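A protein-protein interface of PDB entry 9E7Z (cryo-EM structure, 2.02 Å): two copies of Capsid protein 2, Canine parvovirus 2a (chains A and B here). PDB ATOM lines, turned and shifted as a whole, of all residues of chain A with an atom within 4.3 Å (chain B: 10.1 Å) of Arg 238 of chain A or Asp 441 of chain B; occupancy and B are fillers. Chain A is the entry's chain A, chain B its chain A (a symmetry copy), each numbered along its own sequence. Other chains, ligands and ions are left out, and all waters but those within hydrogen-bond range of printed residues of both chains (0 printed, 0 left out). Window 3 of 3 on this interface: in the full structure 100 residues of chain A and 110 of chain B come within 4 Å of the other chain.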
ATOM      1  N   SER A  98     -27.433   6.725   6.034  1.00  0.00           N
ATOM      2  CA  SER A  98     -26.981   6.846   7.415  1.00  0.00           C
ATOM      3  C   SER A  98     -27.959   7.598   8.309  1.00  0.00           C
ATOM      4  O   SER A  98     -27.938   7.390   9.526  1.00  0.00           O
ATOM      5  CB  SER A  98     -25.617   7.545   7.475  1.00  0.00           C
ATOM      6  OG  SER A  98     -25.707   8.898   7.070  1.00  0.00           O
ATOM      7  N   PRO A 236     -33.803  14.580  12.931  1.00  0.00           N
ATOM      8  CA  PRO A 236     -33.383  13.472  12.068  1.00  0.00           C
ATOM      9  C   PRO A 236     -33.317  12.162  12.834  1.00  0.00           C
ATOM     10  O   PRO A 236     -33.094  12.129  14.046  1.00  0.00           O
ATOM     11  CB  PRO A 236     -31.996  13.902  11.580  1.00  0.00           C
ATOM     12  CG  PRO A 236     -31.503  14.841  12.614  1.00  0.00           C
ATOM     13  CD  PRO A 236     -32.712  15.541  13.167  1.00  0.00           C
ATOM     14  N   CYS A 237     -33.517  11.071  12.105  1.00  0.00           N
ATOM     15  CA  CYS A 237     -33.431   9.728  12.658  1.00  0.00           C
ATOM     16  C   CYS A 237     -32.182   9.039  12.125  1.00  0.00           C
ATOM     17  O   CYS A 237     -31.989   8.948  10.909  1.00  0.00           O
ATOM     18  CB  CYS A 237     -34.676   8.918  12.304  1.00  0.00           C
ATOM     19  SG  CYS A 237     -34.508   7.152  12.564  1.00  0.00           S
ATOM     20  N   ARG A 238     -31.339   8.561  13.034  1.00  0.00           N
ATOM     21  CA  ARG A 238     -30.127   7.853  12.651  1.00  0.00           C
ATOM     22  C   ARG A 238     -30.467   6.472  12.112  1.00  0.00           C
ATOM     23  O   ARG A 238     -31.381   5.804  12.602  1.00  0.00           O
ATOM     24  CB  ARG A 238     -29.179   7.716  13.844  1.00  0.00           C
ATOM     25  CG  ARG A 238     -28.955   8.987  14.652  1.00  0.00           C
ATOM     26  CD  ARG A 238     -28.444  10.138  13.803  1.00  0.00           C
ATOM     27  NE  ARG A 238     -27.033   9.993  13.470  1.00  0.00           N
ATOM     28  CZ  ARG A 238     -26.032  10.350  14.266  1.00  0.00           C
ATOM     29  NH1 ARG A 238     -26.249  10.861  15.467  1.00  0.00           N
ATOM     30  NH2 ARG A 238     -24.782  10.192  13.844  1.00  0.00           N
ATOM     31  N   LEU A 239     -29.723   6.047  11.092  1.00  0.00           N
ATOM     32  CA  LEU A 239     -29.780   4.680  10.592  1.00  0.00           C
ATOM     33  C   LEU A 239     -28.506   3.914  10.932  1.00  0.00           C
ATOM     34  O   LEU A 239     -28.138   2.964  10.242  1.00  0.00           O
ATOM     35  CB  LEU A 239     -30.031   4.667   9.086  1.00  0.00           C
ATOM     36  CG  LEU A 239     -31.366   5.283   8.666  1.00  0.00           C
ATOM     37  CD1 LEU A 239     -31.500   5.308   7.155  1.00  0.00           C
ATOM     38  CD2 LEU A 239     -32.529   4.536   9.305  1.00  0.00           C
ATOM     39  N   THR A 240     -27.820   4.337  11.991  1.00  0.00           N
ATOM     40  CA  THR A 240     -26.669   3.633  12.528  1.00  0.00           C
ATOM     41  C   THR A 240     -26.904   3.379  14.009  1.00  0.00           C
ATOM     42  O   THR A 240     -27.712   4.055  14.649  1.00  0.00           O
ATOM     43  CB  THR A 240     -25.361   4.426  12.342  1.00  0.00           C
ATOM     44  OG1 THR A 240     -25.466   5.696  12.994  1.00  0.00           O
ATOM     45  CG2 THR A 240     -25.057   4.636  10.869  1.00  0.00           C
ATOM     46  N   LEU A 421     -28.087   8.579  25.666  1.00  0.00           N
ATOM     47  CA  LEU A 421     -28.843   7.492  25.061  1.00  0.00           C
ATOM     48  C   LEU A 421     -29.250   7.894  23.652  1.00  0.00           C
ATOM     49  O   LEU A 421     -29.030   9.025  23.215  1.00  0.00           O
ATOM     50  CB  LEU A 421     -30.069   7.125  25.905  1.00  0.00           C
ATOM     51  CG  LEU A 421     -31.062   8.254  26.176  1.00  0.00           C
ATOM     52  CD1 LEU A 421     -32.493   7.761  26.014  1.00  0.00           C
ATOM     53  CD2 LEU A 421     -30.847   8.829  27.563  1.00  0.00           C
ATOM     54  N   ASN A 422     -29.852   6.947  22.943  1.00  0.00           N
ATOM     55  CA  ASN A 422     -30.266   7.144  21.563  1.00  0.00           C
ATOM     56  C   ASN A 422     -31.784   7.115  21.448  1.00  0.00           C
ATOM     57  O   ASN A 422     -32.499   6.677  22.351  1.00  0.00           O
ATOM     58  CB  ASN A 422     -29.650   6.071  20.660  1.00  0.00           C
ATOM     59  CG  ASN A 422     -28.142   6.148  20.615  1.00  0.00           C
ATOM     60  OD1 ASN A 422     -27.572   7.212  20.390  1.00  0.00           O
ATOM     61  ND2 ASN A 422     -27.486   5.016  20.823  1.00  0.00           N
ATOM     62  N   ASN A 423     -32.269   7.599  20.310  1.00  0.00           N
ATOM     63  CA  ASN A 423     -33.682   7.497  19.992  1.00  0.00           C
ATOM     64  C   ASN A 423     -34.023   6.067  19.577  1.00  0.00           C
ATOM     65  O   ASN A 423     -33.152   5.275  19.208  1.00  0.00           O
ATOM     66  CB  ASN A 423     -34.048   8.481  18.882  1.00  0.00           C
ATOM     67  CG  ASN A 423     -35.529   8.802  18.851  1.00  0.00           C
ATOM     68  OD1 ASN A 423     -36.283   8.382  19.725  1.00  0.00           O
ATOM     69  ND2 ASN A 423     -35.953   9.547  17.837  1.00  0.00           N
ATOM     70  N   GLN A 541     -30.807  -0.152  12.004  1.00  0.00           N
ATOM     71  CA  GLN A 541     -29.590   0.541  12.413  1.00  0.00           C
ATOM     72  C   GLN A 541     -28.395  -0.391  12.267  1.00  0.00           C
ATOM     73  O   GLN A 541     -27.578  -0.524  13.184  1.00  0.00           O
ATOM     74  CB  GLN A 541     -29.733   1.064  13.843  1.00  0.00           C
ATOM     75  CG  GLN A 541     -30.782   2.166  13.961  1.00  0.00           C
ATOM     76  CD  GLN A 541     -30.700   2.944  15.260  1.00  0.00           C
ATOM     77  OE1 GLN A 541     -30.087   2.501  16.229  1.00  0.00           O
ATOM     78  NE2 GLN A 541     -31.316   4.117  15.282  1.00  0.00           N
ATOM     79  N   ARG A 545     -21.747   3.210  14.264  1.00  0.00           N
ATOM     80  CA  ARG A 545     -21.106   4.513  14.277  1.00  0.00           C
ATOM     81  C   ARG A 545     -20.367   4.672  15.594  1.00  0.00           C
ATOM     82  O   ARG A 545     -20.758   4.102  16.615  1.00  0.00           O
ATOM     83  CB  ARG A 545     -22.112   5.664  14.077  1.00  0.00           C
ATOM     84  CG  ARG A 545     -22.962   6.020  15.292  1.00  0.00           C
ATOM     85  CD  ARG A 545     -23.616   7.376  15.103  1.00  0.00           C
ATOM     86  NE  ARG A 545     -24.451   7.748  16.239  1.00  0.00           N
ATOM     87  CZ  ARG A 545     -25.653   7.247  16.483  1.00  0.00           C
ATOM     88  NH1 ARG A 545     -26.203   6.347  15.685  1.00  0.00           N
ATOM     89  NH2 ARG A 545     -26.322   7.661  17.554  1.00  0.00           N
ATOM     90  N   GLU B 437     -18.043  15.820  22.463  1.00  0.00           N
ATOM     91  CA  GLU B 437     -19.390  15.443  22.870  1.00  0.00           C
ATOM     92  C   GLU B 437     -19.789  14.115  22.241  1.00  0.00           C
ATOM     93  O   GLU B 437     -19.391  13.790  21.120  1.00  0.00           O
ATOM     94  CB  GLU B 437     -20.391  16.528  22.473  1.00  0.00           C
ATOM     95  CG  GLU B 437     -21.818  16.268  22.924  1.00  0.00           C
ATOM     96  CD  GLU B 437     -21.951  16.154  24.432  1.00  0.00           C
ATOM     97  OE1 GLU B 437     -21.644  15.076  24.981  1.00  0.00           O
ATOM     98  OE2 GLU B 437     -22.367  17.142  25.067  1.00  0.00           O
ATOM     99  N   PHE B 438     -20.592  13.350  22.974  1.00  0.00           N
ATOM    100  CA  PHE B 438     -21.051  12.058  22.484  1.00  0.00           C
ATOM    101  C   PHE B 438     -21.902  12.233  21.235  1.00  0.00           C
ATOM    102  O   PHE B 438     -22.586  13.245  21.064  1.00  0.00           O
ATOM    103  CB  PHE B 438     -21.862  11.337  23.563  1.00  0.00           C
ATOM    104  CG  PHE B 438     -21.041  10.814  24.709  1.00  0.00           C
ATOM    105  CD1 PHE B 438     -19.677  11.048  24.785  1.00  0.00           C
ATOM    106  CD2 PHE B 438     -21.643  10.078  25.713  1.00  0.00           C
ATOM    107  CE1 PHE B 438     -18.937  10.564  25.840  1.00  0.00           C
ATOM    108  CE2 PHE B 438     -20.908   9.592  26.769  1.00  0.00           C
ATOM    109  CZ  PHE B 438     -19.553   9.833  26.835  1.00  0.00           C
ATOM    110  N   ASP B 439     -21.872  11.228  20.366  1.00  0.00           N
ATOM    111  CA  ASP B 439     -22.673  11.218  19.145  1.00  0.00           C
ATOM    112  C   ASP B 439     -23.962  10.430  19.324  1.00  0.00           C
ATOM    113  O   ASP B 439     -24.412   9.727  18.418  1.00  0.00           O
ATOM    114  CB  ASP B 439     -21.853  10.661  17.986  1.00  0.00           C
ATOM    115  CG  ASP B 439     -22.503  10.916  16.637  1.00  0.00           C
ATOM    116  OD1 ASP B 439     -23.375  11.803  16.551  1.00  0.00           O
ATOM    117  OD2 ASP B 439     -22.145  10.224  15.663  1.00  0.00           O
ATOM    118  N   THR B 440     -24.556  10.512  20.509  1.00  0.00           N
ATOM    119  CA  THR B 440     -25.866   9.942  20.771  1.00  0.00           C
ATOM    120  C   THR B 440     -26.947  10.982  20.500  1.00  0.00           C
ATOM    121  O   THR B 440     -26.686  12.187  20.495  1.00  0.00           O
ATOM    122  CB  THR B 440     -25.969   9.454  22.218  1.00  0.00           C
ATOM    123  OG1 THR B 440     -25.669  10.530  23.116  1.00  0.00           O
ATOM    124  CG2 THR B 440     -25.009   8.303  22.469  1.00  0.00           C
ATOM    125  N   ASP B 441     -28.171  10.502  20.273  1.00  0.00           N
ATOM    126  CA  ASP B 441     -29.288  11.415  20.055  1.00  0.00           C
ATOM    127  C   ASP B 441     -29.508  12.305  21.271  1.00  0.00           C
ATOM    128  O   ASP B 441     -29.667  13.524  21.144  1.00  0.00           O
ATOM    129  CB  ASP B 441     -30.558  10.624  19.738  1.00  0.00           C
ATOM    130  CG  ASP B 441     -30.455   9.849  18.442  1.00  0.00           C
ATOM    131  OD1 ASP B 441     -30.498   8.603  18.490  1.00  0.00           O
ATOM    132  OD2 ASP B 441     -30.338  10.489  17.377  1.00  0.00           O
ATOM    133  N   LEU B 442     -29.514  11.712  22.458  1.00  0.00           N
ATOM    134  CA  LEU B 442     -29.670  12.443  23.706  1.00  0.00           C
ATOM    135  C   LEU B 442     -28.316  12.525  24.396  1.00  0.00           C
ATOM    136  O   LEU B 442     -27.670  11.501  24.631  1.00  0.00           O
ATOM    137  CB  LEU B 442     -30.696  11.764  24.611  1.00  0.00           C
ATOM    138  CG  LEU B 442     -32.073  11.544  23.974  1.00  0.00           C
ATOM    139  CD1 LEU B 442     -33.015  10.881  24.962  1.00  0.00           C
ATOM    140  CD2 LEU B 442     -32.657  12.852  23.466  1.00  0.00           C
ATOM    141  N   LYS B 443     -27.893  13.738  24.711  1.00  0.00           N
ATOM    142  CA  LYS B 443     -26.542  13.966  25.186  1.00  0.00           C
ATOM    143  C   LYS B 443     -26.526  14.240  26.686  1.00  0.00           C
ATOM    144  O   LYS B 443     -27.515  14.719  27.247  1.00  0.00           O
ATOM    145  CB  LYS B 443     -25.908  15.143  24.440  1.00  0.00           C
ATOM    146  CG  LYS B 443     -25.810  14.910  22.941  1.00  0.00           C
ATOM    147  CD  LYS B 443     -25.406  16.159  22.196  1.00  0.00           C
ATOM    148  CE  LYS B 443     -25.589  15.988  20.697  1.00  0.00           C
ATOM    149  NZ  LYS B 443     -24.943  14.749  20.190  1.00  0.00           N
ATOM    150  N   PRO B 444     -25.424  13.933  27.366  1.00  0.00           N
ATOM    151  CA  PRO B 444     -25.334  14.260  28.790  1.00  0.00           C
ATOM    152  C   PRO B 444     -25.317  15.766  29.002  1.00  0.00           C
ATOM    153  O   PRO B 444     -24.904  16.535  28.134  1.00  0.00           O
ATOM    154  CB  PRO B 444     -24.013  13.614  29.224  1.00  0.00           C
ATOM    155  CG  PRO B 444     -23.213  13.515  27.982  1.00  0.00           C
ATOM    156  CD  PRO B 444     -24.184  13.322  26.858  1.00  0.00           C
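OD2 of Asp 439 of chain B is in salt-bridge range of NH2 of Arg 238 of chain A, at 3.2 Å.
The backbone carbonyl oxygen (O) of Leu 421 of chain A lies within hydrogen-bond range of the backbone NH (N) of Asp 441 of chain B (3.4 Å).
The backbone carbonyl oxygen (O) of Leu 421 of chain A sits at hydrogen-bond distance from the backbone NH (N) of Leu 442 of chain B (2.8 Å).
OD1 of Asn 422 of chain A lies within hydrogen-bond range of N of Asp 441 of chain B (3.3 Å).
The backbone NH (N) of Asn 423 of chain A sits at hydrogen-bond distance from the side-chain carboxylate (OD1) of Asp 441 of chain B (2.7 Å).
NE of Arg 545 of chain A is in salt-bridge range of OD2 of Asp 439 of chain B, 3.4 Å away.
O of Arg 238 of chain A is in hydrogen-bond range of NE2 of Gln 541 of chain A (3.2 Å).
The guanidinium group of Arg 545 of chain A sits at hydrogen-bond distance from the side-chain hydroxyl of Thr 240 of chain A, 2.9 Å away.
OD1 of Asn 422 of chain A lies within hydrogen-bond range of NH2 of Arg 545 of chain A (3.1 Å).
OG1 of Thr 440 of chain B lies within hydrogen-bond range of O of Leu 442 of chain B, at 2.7 Å.
The backbone carbonyl oxygen (O) of Thr 440 of chain B sits at hydrogen-bond distance from the side-chain amino group (NZ) of Lys 443 of chain B (3.1 Å).
Among the printed residues, merely in contact across the chains: Asn 422 of chain A with Thr 440 of chain B (3.2 Å), Leu 421 of chain A with Thr 440 of chain B (3.2 Å), Arg 238 of chain A with Asp 441 of chain B (3.4 Å) and Arg 545 of chain A with Thr 440 of chain B (3.97 Å).
Arg 238 of chain A touches just these residues of chain B: Asp 439 and Asp 441.
Asp 441 of chain B touches just these residues of chain A: Arg 238 (3.4 Å), Leu 421 (3.4 Å), Asn 422 (3.3 Å) and Asn 423 (2.7 Å).
No residue of chain B comes within 4 Å of Cys 237 of chain A.
No residue of chain B comes within 4 Å of Leu 239 of chain A.
No residue of chain B comes within 4 Å of Thr 240 of chain A.
Of chain B, only Thr 440 and Asp 441 come within 4 Å of Asn 422 of chain A.
Asn 423 of chain A touches just one residue of chain B: Asp 441.
Of the printed residues of chain B, Leu 421 of chain A touches Thr 440, Asp 441 and Leu 442.
Of the printed residues of chain A, Thr 440 of chain B touches Leu 421 (3.2 Å), Asn 422 (3.2 Å) and Arg 545 (3.97 Å).
Printed residues of chain A within 4 Å of Leu 442 of chain B: Leu 421 (2.8 Å).
Printed residues of chain B within 4 Å of Arg 545 of chain A: Asp 439 and Thr 440.
The nearest printed residue of chain B that does not touch Arg 545 of chain A is Asp 441 of chain B (4.3 Å).
Printed residues of chain A that touch a printed residue of chain B: Arg 238, Leu 421, Asn 422, Asn 423 and Arg 545.
Among the printed residues, 10 pairs touch across the chains.
No position is printed for both chains.
Of the 10 pairs that touch across the chains among the printed residues, none has its exchanged pair printed and touching as well.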
